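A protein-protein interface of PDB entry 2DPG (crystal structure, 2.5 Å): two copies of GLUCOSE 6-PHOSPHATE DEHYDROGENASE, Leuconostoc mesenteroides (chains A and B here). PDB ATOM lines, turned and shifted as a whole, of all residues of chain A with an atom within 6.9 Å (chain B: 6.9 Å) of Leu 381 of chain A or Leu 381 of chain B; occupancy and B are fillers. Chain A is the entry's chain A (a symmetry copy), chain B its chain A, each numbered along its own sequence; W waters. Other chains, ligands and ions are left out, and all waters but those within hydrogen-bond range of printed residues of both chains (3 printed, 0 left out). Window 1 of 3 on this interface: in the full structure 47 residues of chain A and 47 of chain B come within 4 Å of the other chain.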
ATOM      1  N   ILE A 197     -11.854  -2.024 -23.485  1.00  0.00           N
ATOM      2  CA  ILE A 197     -12.261  -2.750 -22.280  1.00  0.00           C
ATOM      3  C   ILE A 197     -11.134  -2.999 -21.276  1.00  0.00           C
ATOM      4  O   ILE A 197     -11.400  -3.229 -20.107  1.00  0.00           O
ATOM      5  CB  ILE A 197     -12.983  -4.082 -22.599  1.00  0.00           C
ATOM      6  CG1 ILE A 197     -12.145  -4.944 -23.546  1.00  0.00           C
ATOM      7  CG2 ILE A 197     -14.374  -3.799 -23.163  1.00  0.00           C
ATOM      8  CD1 ILE A 197     -12.670  -6.353 -23.682  1.00  0.00           C
ATOM      9  N   PHE A 198      -9.884  -2.966 -21.736  1.00  0.00           N
ATOM     10  CA  PHE A 198      -8.730  -3.155 -20.858  1.00  0.00           C
ATOM     11  C   PHE A 198      -8.176  -1.800 -20.495  1.00  0.00           C
ATOM     12  O   PHE A 198      -7.868  -1.530 -19.334  1.00  0.00           O
ATOM     13  CB  PHE A 198      -7.655  -3.989 -21.541  1.00  0.00           C
ATOM     14  CG  PHE A 198      -7.988  -5.437 -21.599  1.00  0.00           C
ATOM     15  CD1 PHE A 198      -8.505  -6.077 -20.480  1.00  0.00           C
ATOM     16  CD2 PHE A 198      -7.811  -6.163 -22.766  1.00  0.00           C
ATOM     17  CE1 PHE A 198      -8.843  -7.420 -20.517  1.00  0.00           C
ATOM     18  CE2 PHE A 198      -8.144  -7.508 -22.817  1.00  0.00           C
ATOM     19  CZ  PHE A 198      -8.663  -8.141 -21.688  1.00  0.00           C
ATOM     20  N   ILE A 349      -1.969  -9.838 -14.372  1.00  0.00           N
ATOM     21  CA  ILE A 349      -2.749  -8.725 -13.854  1.00  0.00           C
ATOM     22  C   ILE A 349      -3.959  -9.328 -13.163  1.00  0.00           C
ATOM     23  O   ILE A 349      -4.791  -9.991 -13.792  1.00  0.00           O
ATOM     24  CB  ILE A 349      -3.176  -7.724 -14.968  1.00  0.00           C
ATOM     25  CG1 ILE A 349      -1.944  -7.050 -15.574  1.00  0.00           C
ATOM     26  CG2 ILE A 349      -4.121  -6.672 -14.402  1.00  0.00           C
ATOM     27  CD1 ILE A 349      -1.556  -7.622 -16.912  1.00  0.00           C
ATOM     28  N   PHE A 351      -7.349  -8.925 -11.419  1.00  0.00           N
ATOM     29  CA  PHE A 351      -8.489  -8.019 -11.343  1.00  0.00           C
ATOM     30  C   PHE A 351      -9.311  -8.296 -10.099  1.00  0.00           C
ATOM     31  O   PHE A 351      -9.426  -9.448  -9.666  1.00  0.00           O
ATOM     32  CB  PHE A 351      -9.376  -8.173 -12.581  1.00  0.00           C
ATOM     33  CG  PHE A 351      -8.738  -7.681 -13.852  1.00  0.00           C
ATOM     34  CD1 PHE A 351      -8.588  -6.319 -14.092  1.00  0.00           C
ATOM     35  CD2 PHE A 351      -8.295  -8.579 -14.814  1.00  0.00           C
ATOM     36  CE1 PHE A 351      -8.003  -5.862 -15.274  1.00  0.00           C
ATOM     37  CE2 PHE A 351      -7.708  -8.134 -16.000  1.00  0.00           C
ATOM     38  CZ  PHE A 351      -7.563  -6.769 -16.229  1.00  0.00           C
ATOM     39  N   ALA A 367     -10.389 -12.335 -11.740  1.00  0.00           N
ATOM     40  CA  ALA A 367     -10.020 -12.599 -13.126  1.00  0.00           C
ATOM     41  C   ALA A 367      -8.554 -12.230 -13.290  1.00  0.00           C
ATOM     42  O   ALA A 367      -8.071 -11.302 -12.640  1.00  0.00           O
ATOM     43  CB  ALA A 367     -10.873 -11.768 -14.061  1.00  0.00           C
ATOM     44  N   VAL A 368      -7.848 -12.941 -14.162  1.00  0.00           N
ATOM     45  CA  VAL A 368      -6.431 -12.684 -14.378  1.00  0.00           C
ATOM     46  C   VAL A 368      -6.064 -12.566 -15.851  1.00  0.00           C
ATOM     47  O   VAL A 368      -6.507 -13.367 -16.669  1.00  0.00           O
ATOM     48  CB  VAL A 368      -5.583 -13.827 -13.768  1.00  0.00           C
ATOM     49  CG1 VAL A 368      -4.099 -13.493 -13.799  1.00  0.00           C
ATOM     50  CG2 VAL A 368      -6.033 -14.092 -12.357  1.00  0.00           C
ATOM     51  N   LEU A 369      -5.274 -11.551 -16.187  1.00  0.00           N
ATOM     52  CA  LEU A 369      -4.793 -11.371 -17.547  1.00  0.00           C
ATOM     53  C   LEU A 369      -3.308 -11.697 -17.476  1.00  0.00           C
ATOM     54  O   LEU A 369      -2.511 -10.935 -16.915  1.00  0.00           O
ATOM     55  CB  LEU A 369      -4.994  -9.929 -18.025  1.00  0.00           C
ATOM     56  CG  LEU A 369      -4.316  -9.553 -19.360  1.00  0.00           C
ATOM     57  CD1 LEU A 369      -4.664 -10.560 -20.452  1.00  0.00           C
ATOM     58  CD2 LEU A 369      -4.713  -8.136 -19.795  1.00  0.00           C
ATOM     59  N   SER A 370      -2.947 -12.861 -17.990  1.00  0.00           N
ATOM     60  CA  SER A 370      -1.561 -13.295 -17.986  1.00  0.00           C
ATOM     61  C   SER A 370      -0.910 -13.072 -19.343  1.00  0.00           C
ATOM     62  O   SER A 370      -1.524 -13.305 -20.385  1.00  0.00           O
ATOM     63  CB  SER A 370      -1.481 -14.778 -17.645  1.00  0.00           C
ATOM     64  OG  SER A 370      -2.076 -15.056 -16.388  1.00  0.00           O
ATOM     65  N   ILE A 379      -0.864 -15.439 -24.297  1.00  0.00           N
ATOM     66  CA  ILE A 379      -1.743 -14.507 -23.591  1.00  0.00           C
ATOM     67  C   ILE A 379      -2.942 -15.307 -23.101  1.00  0.00           C
ATOM     68  O   ILE A 379      -3.586 -16.021 -23.875  1.00  0.00           O
ATOM     69  CB  ILE A 379      -2.243 -13.355 -24.510  1.00  0.00           C
ATOM     70  CG1 ILE A 379      -1.056 -12.547 -25.028  1.00  0.00           C
ATOM     71  CG2 ILE A 379      -3.216 -12.444 -23.755  1.00  0.00           C
ATOM     72  CD1 ILE A 379      -1.437 -11.459 -25.986  1.00  0.00           C
ATOM     73  N   GLU A 380      -3.212 -15.221 -21.805  1.00  0.00           N
ATOM     74  CA  GLU A 380      -4.326 -15.941 -21.216  1.00  0.00           C
ATOM     75  C   GLU A 380      -5.216 -15.022 -20.404  1.00  0.00           C
ATOM     76  O   GLU A 380      -4.765 -14.020 -19.850  1.00  0.00           O
ATOM     77  CB  GLU A 380      -3.820 -17.070 -20.332  1.00  0.00           C
ATOM     78  CG  GLU A 380      -3.168 -18.184 -21.102  1.00  0.00           C
ATOM     79  CD  GLU A 380      -2.644 -19.264 -20.187  1.00  0.00           C
ATOM     80  OE1 GLU A 380      -3.473 -19.918 -19.506  1.00  0.00           O
ATOM     81  OE2 GLU A 380      -1.404 -19.449 -20.144  1.00  0.00           O
ATOM     82  N   LEU A 381      -6.490 -15.375 -20.333  1.00  0.00           N
ATOM     83  CA  LEU A 381      -7.449 -14.586 -19.598  1.00  0.00           C
ATOM     84  C   LEU A 381      -8.395 -15.525 -18.869  1.00  0.00           C
ATOM     85  O   LEU A 381      -9.253 -16.159 -19.478  1.00  0.00           O
ATOM     86  CB  LEU A 381      -8.215 -13.666 -20.550  1.00  0.00           C
ATOM     87  CG  LEU A 381      -9.248 -12.708 -19.957  1.00  0.00           C
ATOM     88  CD1 LEU A 381      -8.593 -11.670 -19.037  1.00  0.00           C
ATOM     89  CD2 LEU A 381      -9.957 -12.022 -21.092  1.00  0.00           C
ATOM     90  N   LYS A 382      -8.173 -15.655 -17.566  1.00  0.00           N
ATOM     91  CA  LYS A 382      -8.979 -16.503 -16.700  1.00  0.00           C
ATOM     92  C   LYS A 382     -10.189 -15.673 -16.302  1.00  0.00           C
ATOM     93  O   LYS A 382     -10.046 -14.646 -15.629  1.00  0.00           O
ATOM     94  CB  LYS A 382      -8.160 -16.874 -15.469  1.00  0.00           C
ATOM     95  CG  LYS A 382      -8.822 -17.822 -14.502  1.00  0.00           C
ATOM     96  CD  LYS A 382      -8.065 -17.848 -13.168  1.00  0.00           C
ATOM     97  CE  LYS A 382      -6.810 -18.729 -13.208  1.00  0.00           C
ATOM     98  NZ  LYS A 382      -5.739 -18.321 -14.177  1.00  0.00           N
ATOM     99  N   LEU A 383     -11.368 -16.092 -16.759  1.00  0.00           N
ATOM    100  CA  LEU A 383     -12.630 -15.388 -16.490  1.00  0.00           C
ATOM    101  C   LEU A 383     -13.600 -16.248 -15.691  1.00  0.00           C
ATOM    102  O   LEU A 383     -13.433 -17.464 -15.609  1.00  0.00           O
ATOM    103  CB  LEU A 383     -13.319 -14.996 -17.809  1.00  0.00           C
ATOM    104  CG  LEU A 383     -12.715 -13.960 -18.760  1.00  0.00           C
ATOM    105  CD1 LEU A 383     -13.445 -13.994 -20.087  1.00  0.00           C
ATOM    106  CD2 LEU A 383     -12.794 -12.580 -18.139  1.00  0.00           C
ATOM    107  N   ILE A 397     -12.665 -20.182 -16.116  1.00  0.00           N
ATOM    108  CA  ILE A 397     -12.191 -20.856 -17.318  1.00  0.00           C
ATOM    109  C   ILE A 397     -11.060 -19.999 -17.904  1.00  0.00           C
ATOM    110  O   ILE A 397     -10.943 -18.812 -17.585  1.00  0.00           O
ATOM    111  CB  ILE A 397     -13.318 -21.038 -18.360  1.00  0.00           C
ATOM    112  CG1 ILE A 397     -13.932 -19.683 -18.703  1.00  0.00           C
ATOM    113  CG2 ILE A 397     -14.382 -22.001 -17.823  1.00  0.00           C
ATOM    114  CD1 ILE A 397     -14.811 -19.718 -19.900  1.00  0.00           C
ATOM    115  N   ASP A 398     -10.212 -20.600 -18.727  1.00  0.00           N
ATOM    116  CA  ASP A 398      -9.105 -19.862 -19.319  1.00  0.00           C
ATOM    117  C   ASP A 398      -9.203 -19.746 -20.826  1.00  0.00           C
ATOM    118  O   ASP A 398      -9.296 -20.755 -21.521  1.00  0.00           O
ATOM    119  CB  ASP A 398      -7.768 -20.510 -18.944  1.00  0.00           C
ATOM    120  CG  ASP A 398      -7.411 -20.308 -17.483  1.00  0.00           C
ATOM    121  OD1 ASP A 398      -7.951 -21.048 -16.629  1.00  0.00           O
ATOM    122  OD2 ASP A 398      -6.585 -19.412 -17.188  1.00  0.00           O
ATOM    123  N   LEU A 399      -9.260 -18.509 -21.312  1.00  0.00           N
ATOM    124  CA  LEU A 399      -9.290 -18.230 -22.737  1.00  0.00           C
ATOM    125  C   LEU A 399      -7.818 -17.988 -23.049  1.00  0.00           C
ATOM    126  O   LEU A 399      -7.200 -17.099 -22.456  1.00  0.00           O
ATOM    127  CB  LEU A 399     -10.060 -16.940 -23.037  1.00  0.00           C
ATOM    128  CG  LEU A 399     -11.504 -16.743 -22.579  1.00  0.00           C
ATOM    129  CD1 LEU A 399     -12.042 -15.458 -23.188  1.00  0.00           C
ATOM    130  CD2 LEU A 399     -12.344 -17.911 -23.004  1.00  0.00           C
ATOM    131  N   GLY A 400      -7.244 -18.759 -23.962  1.00  0.00           N
ATOM    132  CA  GLY A 400      -5.842 -18.556 -24.260  1.00  0.00           C
ATOM    133  C   GLY A 400      -5.475 -18.391 -25.718  1.00  0.00           C
ATOM    134  O   GLY A 400      -6.298 -18.614 -26.604  1.00  0.00           O
ATOM    135  N   TRP A 401      -4.243 -17.939 -25.945  1.00  0.00           N
ATOM    136  CA  TRP A 401      -3.677 -17.749 -27.277  1.00  0.00           C
ATOM    137  C   TRP A 401      -2.156 -17.908 -27.173  1.00  0.00           C
ATOM    138  O   TRP A 401      -1.537 -17.418 -26.230  1.00  0.00           O
ATOM    139  CB  TRP A 401      -4.033 -16.372 -27.833  1.00  0.00           C
ATOM    140  CG  TRP A 401      -3.336 -16.047 -29.124  1.00  0.00           C
ATOM    141  CD1 TRP A 401      -3.786 -16.294 -30.400  1.00  0.00           C
ATOM    142  CD2 TRP A 401      -2.072 -15.385 -29.267  1.00  0.00           C
ATOM    143  NE1 TRP A 401      -2.880 -15.819 -31.321  1.00  0.00           N
ATOM    144  CE2 TRP A 401      -1.820 -15.256 -30.654  1.00  0.00           C
ATOM    145  CE3 TRP A 401      -1.126 -14.884 -28.356  1.00  0.00           C
ATOM    146  CZ2 TRP A 401      -0.665 -14.647 -31.148  1.00  0.00           C
ATOM    147  CZ3 TRP A 401       0.023 -14.281 -28.852  1.00  0.00           C
ATOM    148  CH2 TRP A 401       0.243 -14.169 -30.234  1.00  0.00           C
ATOM    149  N   ILE B 197     -14.993  -6.376 -15.761  1.00  0.00           N
ATOM    150  CA  ILE B 197     -14.544  -5.767 -17.015  1.00  0.00           C
ATOM    151  C   ILE B 197     -15.540  -5.880 -18.170  1.00  0.00           C
ATOM    152  O   ILE B 197     -15.470  -5.107 -19.113  1.00  0.00           O
ATOM    153  CB  ILE B 197     -13.156  -6.285 -17.468  1.00  0.00           C
ATOM    154  CG1 ILE B 197     -13.135  -7.815 -17.518  1.00  0.00           C
ATOM    155  CG2 ILE B 197     -12.069  -5.727 -16.553  1.00  0.00           C
ATOM    156  CD1 ILE B 197     -11.905  -8.365 -18.200  1.00  0.00           C
ATOM    157  N   PHE B 198     -16.456  -6.846 -18.099  1.00  0.00           N
ATOM    158  CA  PHE B 198     -17.478  -7.021 -19.129  1.00  0.00           C
ATOM    159  C   PHE B 198     -18.754  -6.371 -18.655  1.00  0.00           C
ATOM    160  O   PHE B 198     -19.416  -5.654 -19.405  1.00  0.00           O
ATOM    161  CB  PHE B 198     -17.722  -8.499 -19.410  1.00  0.00           C
ATOM    162  CG  PHE B 198     -16.642  -9.126 -20.218  1.00  0.00           C
ATOM    163  CD1 PHE B 198     -16.133  -8.466 -21.328  1.00  0.00           C
ATOM    164  CD2 PHE B 198     -16.116 -10.358 -19.868  1.00  0.00           C
ATOM    165  CE1 PHE B 198     -15.112  -9.021 -22.084  1.00  0.00           C
ATOM    166  CE2 PHE B 198     -15.094 -10.927 -20.614  1.00  0.00           C
ATOM    167  CZ  PHE B 198     -14.589 -10.255 -21.728  1.00  0.00           C
ATOM    168  N   ILE B 349     -20.702 -10.173 -29.718  1.00  0.00           N
ATOM    169  CA  ILE B 349     -20.810  -8.816 -29.205  1.00  0.00           C
ATOM    170  C   ILE B 349     -19.667  -8.029 -29.819  1.00  0.00           C
ATOM    171  O   ILE B 349     -18.490  -8.326 -29.591  1.00  0.00           O
ATOM    172  CB  ILE B 349     -20.763  -8.759 -27.650  1.00  0.00           C
ATOM    173  CG1 ILE B 349     -21.984  -9.466 -27.058  1.00  0.00           C
ATOM    174  CG2 ILE B 349     -20.718  -7.313 -27.173  1.00  0.00           C
ATOM    175  CD1 ILE B 349     -21.671 -10.843 -26.533  1.00  0.00           C
ATOM    176  N   PHE B 351     -17.574  -4.826 -30.059  1.00  0.00           N
ATOM    177  CA  PHE B 351     -17.178  -3.665 -29.273  1.00  0.00           C
ATOM    178  C   PHE B 351     -16.652  -2.562 -30.172  1.00  0.00           C
ATOM    179  O   PHE B 351     -16.024  -2.838 -31.201  1.00  0.00           O
ATOM    180  CB  PHE B 351     -16.097  -4.049 -28.260  1.00  0.00           C
ATOM    181  CG  PHE B 351     -16.587  -4.952 -27.159  1.00  0.00           C
ATOM    182  CD1 PHE B 351     -17.403  -4.461 -26.146  1.00  0.00           C
ATOM    183  CD2 PHE B 351     -16.225  -6.293 -27.132  1.00  0.00           C
ATOM    184  CE1 PHE B 351     -17.853  -5.296 -25.122  1.00  0.00           C
ATOM    185  CE2 PHE B 351     -16.668  -7.137 -26.112  1.00  0.00           C
ATOM    186  CZ  PHE B 351     -17.485  -6.635 -25.104  1.00  0.00           C
ATOM    187  N   ALA B 367     -13.181  -5.176 -31.307  1.00  0.00           N
ATOM    188  CA  ALA B 367     -13.012  -6.408 -30.545  1.00  0.00           C
ATOM    189  C   ALA B 367     -14.354  -7.125 -30.526  1.00  0.00           C
ATOM    190  O   ALA B 367     -15.402  -6.479 -30.520  1.00  0.00           O
ATOM    191  CB  ALA B 367     -12.572  -6.093 -29.131  1.00  0.00           C
ATOM    192  N   VAL B 368     -14.326  -8.454 -30.504  1.00  0.00           N
ATOM    193  CA  VAL B 368     -15.554  -9.237 -30.508  1.00  0.00           C
ATOM    194  C   VAL B 368     -15.574 -10.320 -29.438  1.00  0.00           C
ATOM    195  O   VAL B 368     -14.589 -11.026 -29.248  1.00  0.00           O
ATOM    196  CB  VAL B 368     -15.743  -9.924 -31.882  1.00  0.00           C
ATOM    197  CG1 VAL B 368     -17.110 -10.584 -31.986  1.00  0.00           C
ATOM    198  CG2 VAL B 368     -15.561  -8.915 -32.982  1.00  0.00           C
ATOM    199  N   LEU B 369     -16.690 -10.426 -28.723  1.00  0.00           N
ATOM    200  CA  LEU B 369     -16.862 -11.467 -27.722  1.00  0.00           C
ATOM    201  C   LEU B 369     -17.888 -12.415 -28.324  1.00  0.00           C
ATOM    202  O   LEU B 369     -19.078 -12.089 -28.431  1.00  0.00           O
ATOM    203  CB  LEU B 369     -17.386 -10.892 -26.402  1.00  0.00           C
ATOM    204  CG  LEU B 369     -17.830 -11.919 -25.339  1.00  0.00           C
ATOM    205  CD1 LEU B 369     -16.745 -12.964 -25.103  1.00  0.00           C
ATOM    206  CD2 LEU B 369     -18.194 -11.221 -24.022  1.00  0.00           C
ATOM    207  N   SER B 370     -17.417 -13.566 -28.776  1.00  0.00           N
ATOM    208  CA  SER B 370     -18.290 -14.560 -29.376  1.00  0.00           C
ATOM    209  C   SER B 370     -18.622 -15.669 -28.388  1.00  0.00           C
ATOM    210  O   SER B 370     -17.762 -16.121 -27.631  1.00  0.00           O
ATOM    211  CB  SER B 370     -17.615 -15.179 -30.593  1.00  0.00           C
ATOM    212  OG  SER B 370     -17.273 -14.194 -31.556  1.00  0.00           O
ATOM    213  N   ILE B 379     -16.213 -20.130 -26.282  1.00  0.00           N
ATOM    214  CA  ILE B 379     -16.185 -18.695 -26.001  1.00  0.00           C
ATOM    215  C   ILE B 379     -14.896 -18.148 -26.597  1.00  0.00           C
ATOM    216  O   ILE B 379     -13.807 -18.669 -26.337  1.00  0.00           O
ATOM    217  CB  ILE B 379     -16.209 -18.392 -24.475  1.00  0.00           C
ATOM    218  CG1 ILE B 379     -17.486 -18.947 -23.852  1.00  0.00           C
ATOM    219  CG2 ILE B 379     -16.104 -16.885 -24.222  1.00  0.00           C
ATOM    220  CD1 ILE B 379     -17.561 -18.768 -22.365  1.00  0.00           C
ATOM    221  N   GLU B 380     -15.025 -17.123 -27.429  1.00  0.00           N
ATOM    222  CA  GLU B 380     -13.870 -16.515 -28.065  1.00  0.00           C
ATOM    223  C   GLU B 380     -13.850 -15.014 -27.867  1.00  0.00           C
ATOM    224  O   GLU B 380     -14.892 -14.373 -27.736  1.00  0.00           O
ATOM    225  CB  GLU B 380     -13.856 -16.833 -29.552  1.00  0.00           C
ATOM    226  CG  GLU B 380     -13.587 -18.282 -29.852  1.00  0.00           C
ATOM    227  CD  GLU B 380     -13.621 -18.562 -31.334  1.00  0.00           C
ATOM    228  OE1 GLU B 380     -12.753 -18.018 -32.061  1.00  0.00           O
ATOM    229  OE2 GLU B 380     -14.522 -19.317 -31.769  1.00  0.00           O
ATOM    230  N   LEU B 381     -12.651 -14.455 -27.852  1.00  0.00           N
ATOM    231  CA  LEU B 381     -12.487 -13.033 -27.665  1.00  0.00           C
ATOM    232  C   LEU B 381     -11.378 -12.547 -28.583  1.00  0.00           C
ATOM    233  O   LEU B 381     -10.200 -12.802 -28.345  1.00  0.00           O
ATOM    234  CB  LEU B 381     -12.162 -12.728 -26.202  1.00  0.00           C
ATOM    235  CG  LEU B 381     -11.999 -11.266 -25.786  1.00  0.00           C
ATOM    236  CD1 LEU B 381     -13.308 -10.484 -25.946  1.00  0.00           C
ATOM    237  CD2 LEU B 381     -11.547 -11.235 -24.351  1.00  0.00           C
ATOM    238  N   LYS B 382     -11.784 -11.903 -29.672  1.00  0.00           N
ATOM    239  CA  LYS B 382     -10.870 -11.358 -30.664  1.00  0.00           C
ATOM    240  C   LYS B 382     -10.449  -9.992 -30.145  1.00  0.00           C
ATOM    241  O   LYS B 382     -11.285  -9.091 -30.015  1.00  0.00           O
ATOM    242  CB  LYS B 382     -11.605 -11.220 -31.992  1.00  0.00           C
ATOM    243  CG  LYS B 382     -10.774 -10.742 -33.155  1.00  0.00           C
ATOM    244  CD  LYS B 382     -11.674 -10.320 -34.324  1.00  0.00           C
ATOM    245  CE  LYS B 382     -12.184 -11.510 -35.148  1.00  0.00           C
ATOM    246  NZ  LYS B 382     -13.044 -12.503 -34.423  1.00  0.00           N
ATOM    247  N   LEU B 383      -9.168  -9.858 -29.807  1.00  0.00           N
ATOM    248  CA  LEU B 383      -8.607  -8.612 -29.263  1.00  0.00           C
ATOM    249  C   LEU B 383      -7.539  -8.025 -30.177  1.00  0.00           C
ATOM    250  O   LEU B 383      -7.020  -8.715 -31.053  1.00  0.00           O
ATOM    251  CB  LEU B 383      -7.966  -8.867 -27.888  1.00  0.00           C
ATOM    252  CG  LEU B 383      -8.804  -9.255 -26.667  1.00  0.00           C
ATOM    253  CD1 LEU B 383      -7.895  -9.720 -25.547  1.00  0.00           C
ATOM    254  CD2 LEU B 383      -9.646  -8.077 -26.219  1.00  0.00           C
ATOM    255  N   ILE B 397      -6.019 -10.917 -32.599  1.00  0.00           N
ATOM    256  CA  ILE B 397      -5.751 -12.308 -32.258  1.00  0.00           C
ATOM    257  C   ILE B 397      -6.995 -12.848 -31.541  1.00  0.00           C
ATOM    258  O   ILE B 397      -7.817 -12.075 -31.041  1.00  0.00           O
ATOM    259  CB  ILE B 397      -4.507 -12.450 -31.351  1.00  0.00           C
ATOM    260  CG1 ILE B 397      -4.684 -11.607 -30.091  1.00  0.00           C
ATOM    261  CG2 ILE B 397      -3.246 -12.034 -32.116  1.00  0.00           C
ATOM    262  CD1 ILE B 397      -3.685 -11.906 -29.034  1.00  0.00           C
ATOM    263  N   ASP B 398      -7.155 -14.164 -31.517  1.00  0.00           N
ATOM    264  CA  ASP B 398      -8.312 -14.760 -30.866  1.00  0.00           C
ATOM    265  C   ASP B 398      -7.951 -15.609 -29.664  1.00  0.00           C
ATOM    266  O   ASP B 398      -7.160 -16.542 -29.779  1.00  0.00           O
ATOM    267  CB  ASP B 398      -9.112 -15.604 -31.863  1.00  0.00           C
ATOM    268  CG  ASP B 398      -9.846 -14.758 -32.887  1.00  0.00           C
ATOM    269  OD1 ASP B 398      -9.202 -14.308 -33.862  1.00  0.00           O
ATOM    270  OD2 ASP B 398     -11.072 -14.547 -32.720  1.00  0.00           O
ATOM    271  N   LEU B 399      -8.476 -15.227 -28.503  1.00  0.00           N
ATOM    272  CA  LEU B 399      -8.278 -15.973 -27.272  1.00  0.00           C
ATOM    273  C   LEU B 399      -9.519 -16.856 -27.229  1.00  0.00           C
ATOM    274  O   LEU B 399     -10.642 -16.343 -27.236  1.00  0.00           O
ATOM    275  CB  LEU B 399      -8.303 -15.051 -26.050  1.00  0.00           C
ATOM    276  CG  LEU B 399      -7.360 -13.856 -25.928  1.00  0.00           C
ATOM    277  CD1 LEU B 399      -7.499 -13.262 -24.534  1.00  0.00           C
ATOM    278  CD2 LEU B 399      -5.944 -14.289 -26.170  1.00  0.00           C
ATOM    279  N   GLY B 400      -9.343 -18.169 -27.184  1.00  0.00           N
ATOM    280  CA  GLY B 400     -10.511 -19.025 -27.159  1.00  0.00           C
ATOM    281  C   GLY B 400     -10.561 -20.073 -26.069  1.00  0.00           C
ATOM    282  O   GLY B 400      -9.573 -20.305 -25.374  1.00  0.00           O
ATOM    283  N   TRP B 401     -11.745 -20.657 -25.897  1.00  0.00           N
ATOM    284  CA  TRP B 401     -11.998 -21.720 -24.929  1.00  0.00           C
ATOM    285  C   TRP B 401     -13.152 -22.578 -25.457  1.00  0.00           C
ATOM    286  O   TRP B 401     -14.136 -22.055 -25.977  1.00  0.00           O
ATOM    287  CB  TRP B 401     -12.343 -21.144 -23.559  1.00  0.00           C
ATOM    288  CG  TRP B 401     -12.785 -22.181 -22.565  1.00  0.00           C
ATOM    289  CD1 TRP B 401     -11.994 -22.882 -21.685  1.00  0.00           C
ATOM    290  CD2 TRP B 401     -14.130 -22.616 -22.327  1.00  0.00           C
ATOM    291  NE1 TRP B 401     -12.771 -23.718 -20.914  1.00  0.00           N
ATOM    292  CE2 TRP B 401     -14.084 -23.574 -21.286  1.00  0.00           C
ATOM    293  CE3 TRP B 401     -15.375 -22.287 -22.892  1.00  0.00           C
ATOM    294  CZ2 TRP B 401     -15.231 -24.203 -20.800  1.00  0.00           C
ATOM    295  CZ3 TRP B 401     -16.514 -22.916 -22.407  1.00  0.00           C
ATOM    296  CH2 TRP B 401     -16.434 -23.863 -21.373  1.00  0.00           C
HETATM  297  O   HOH W   1     -14.000  -2.600 -18.955  1.00  0.00           O
HETATM  298  O   HOH W   2      -5.028 -15.636 -33.387  1.00  0.00           O
HETATM  299  O   HOH W   3     -10.673 -23.757 -18.788  1.00  0.00           O
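Ile 349 of chain A touches none of the printed residues of chain B. Leu 381 of chain A touches just one residue of chain B: Leu 381. Printed residues of chain B within 4 Å of Leu 383 of chain A: Phe 198. Printed residues of chain B within 4 Å of Trp 401 of chain A: Ile 397, Asp 398 and Leu 399. Leu 381 of chain B touches just one residue of chain A: Leu 381. Printed residues of chain A within 4 Å of Asp 398 of chain B: Gly 400 (3.9 Å) and Trp 401 (3.4 Å). The nearest residue of chain B that does not touch Leu 381 of chain A is Leu 399 of chain B (4.1 Å). The nearest residue of chain A that does not touch Leu 381 of chain B is Leu 399 of chain A (4.1 Å).
Leu 381 of chain B touches its own counterpart, Leu 381 of chain A. Asp 398 of chain A touches Gly 400 of chain B, and with the chains exchanged Gly 400 of chain A touches Asp 398 of chain B. Leu 399 of chain A touches Gly 400 of chain B, and with the chains exchanged Gly 400 of chain A touches Leu 399 of chain B. Positions printed for both chains: 197, 198, 349, 351, 367, 368, 369, 370, 379, 380, 381, 382, 383, 397, 398, 399, 400 and 401. Of the 21 pairs that touch across the chains among the printed residues, 21 have their exchanged pair printed and touching as well.
The backbone carbonyl oxygen of Gly 400 of chain A sits at hydrogen-bond distance from the backbone NH of Gly 400 of chain B (3.1 Å).
Phe 198 of chain B touches Ile 197 of chain A (CE1 to CD1, 3.95 Å). Phe 198 of chain A touches Ile 197 of chain B. Phe 198 of chain A touches Leu 383 of chain B (CE2 to CD1, 3.5 Å). Ile 397 of chain B touches Ile 379 of chain A (CD1 to CD1, 3.8 Å). Leu 381 of chain A touches Leu 381 of chain B (CD2 to CD2, 3.7 Å). Ile 397 of chain A touches Trp 401 of chain B (CB to NE1, 3.7 Å). Gly 400 of chain B touches Asp 398 of chain A (O to O, 3.9 Å). Asp 398 of chain A touches Trp 401 of chain B (O to CD1, 3.4 Å). Leu 399 of chain A touches Ile 379 of chain B (CD2 to O, 3.7 Å). Trp 401 of chain A touches Asp 398 of chain B (CD1 to O, 3.4 Å).
Of the 18 printed residues of chain B, 10 touch a printed residue of chain A. Hydrophobic or aromatic side chains of chain B within 4 Å of the printed part of chain A: Ile 197, Phe 198, Ile 379, Leu 381, Leu 383, Ile 397, Leu 399 and Trp 401. Of the 18 printed residues of chain A, 10 touch a printed residue of chain B. Hydrophobic or aromatic side chains of chain A within 4 Å of the printed part of chain B: Ile 197, Phe 198, Ile 379, Leu 381, Leu 383, Ile 397, Leu 399 and Trp 401. Among the printed residues, 21 pairs touch across the chains. Among the printed residues, no Asp or Glu carboxylate lies within 4 Å of a Lys or Arg side-chain nitrogen of the other chain.
The side-chain amino group (NZ) of Lys 382 of chain B is in salt-bridge range of the side-chain carboxylate (OD2) of Asp 398 of chain B (3.3 Å). The backbone NH (N) of Ile 397 of chain B is in hydrogen-bond range of the backbone carbonyl oxygen (O) of Leu 383 of chain B (2.9 Å). N of Ile 397 of chain A sits at hydrogen-bond distance from O of Leu 383 of chain A. The backbone carbonyl oxygen of Leu 399 of chain A lies within hydrogen-bond range of the backbone NH of Leu 381 of chain A, at 2.8 Å. N of Ile 379 of chain B sits at hydrogen-bond distance from O of Trp 401 of chain B, at 2.8 Å.
Water W1 bridges the backbone carbonyl oxygen of Ile 197 of chain B (2.9 Å) and the backbone carbonyl oxygen of Ile 197 of chain A (2.9 Å). Water W2 lies within hydrogen-bond range of NE1 of Trp 401 of chain A (3.0 Å) and N of Asp 398 of chain B (3.2 Å). Water W3 bridges the indole nitrogen of Trp 401 of chain B and the backbone NH of Asp 398 of chain A.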
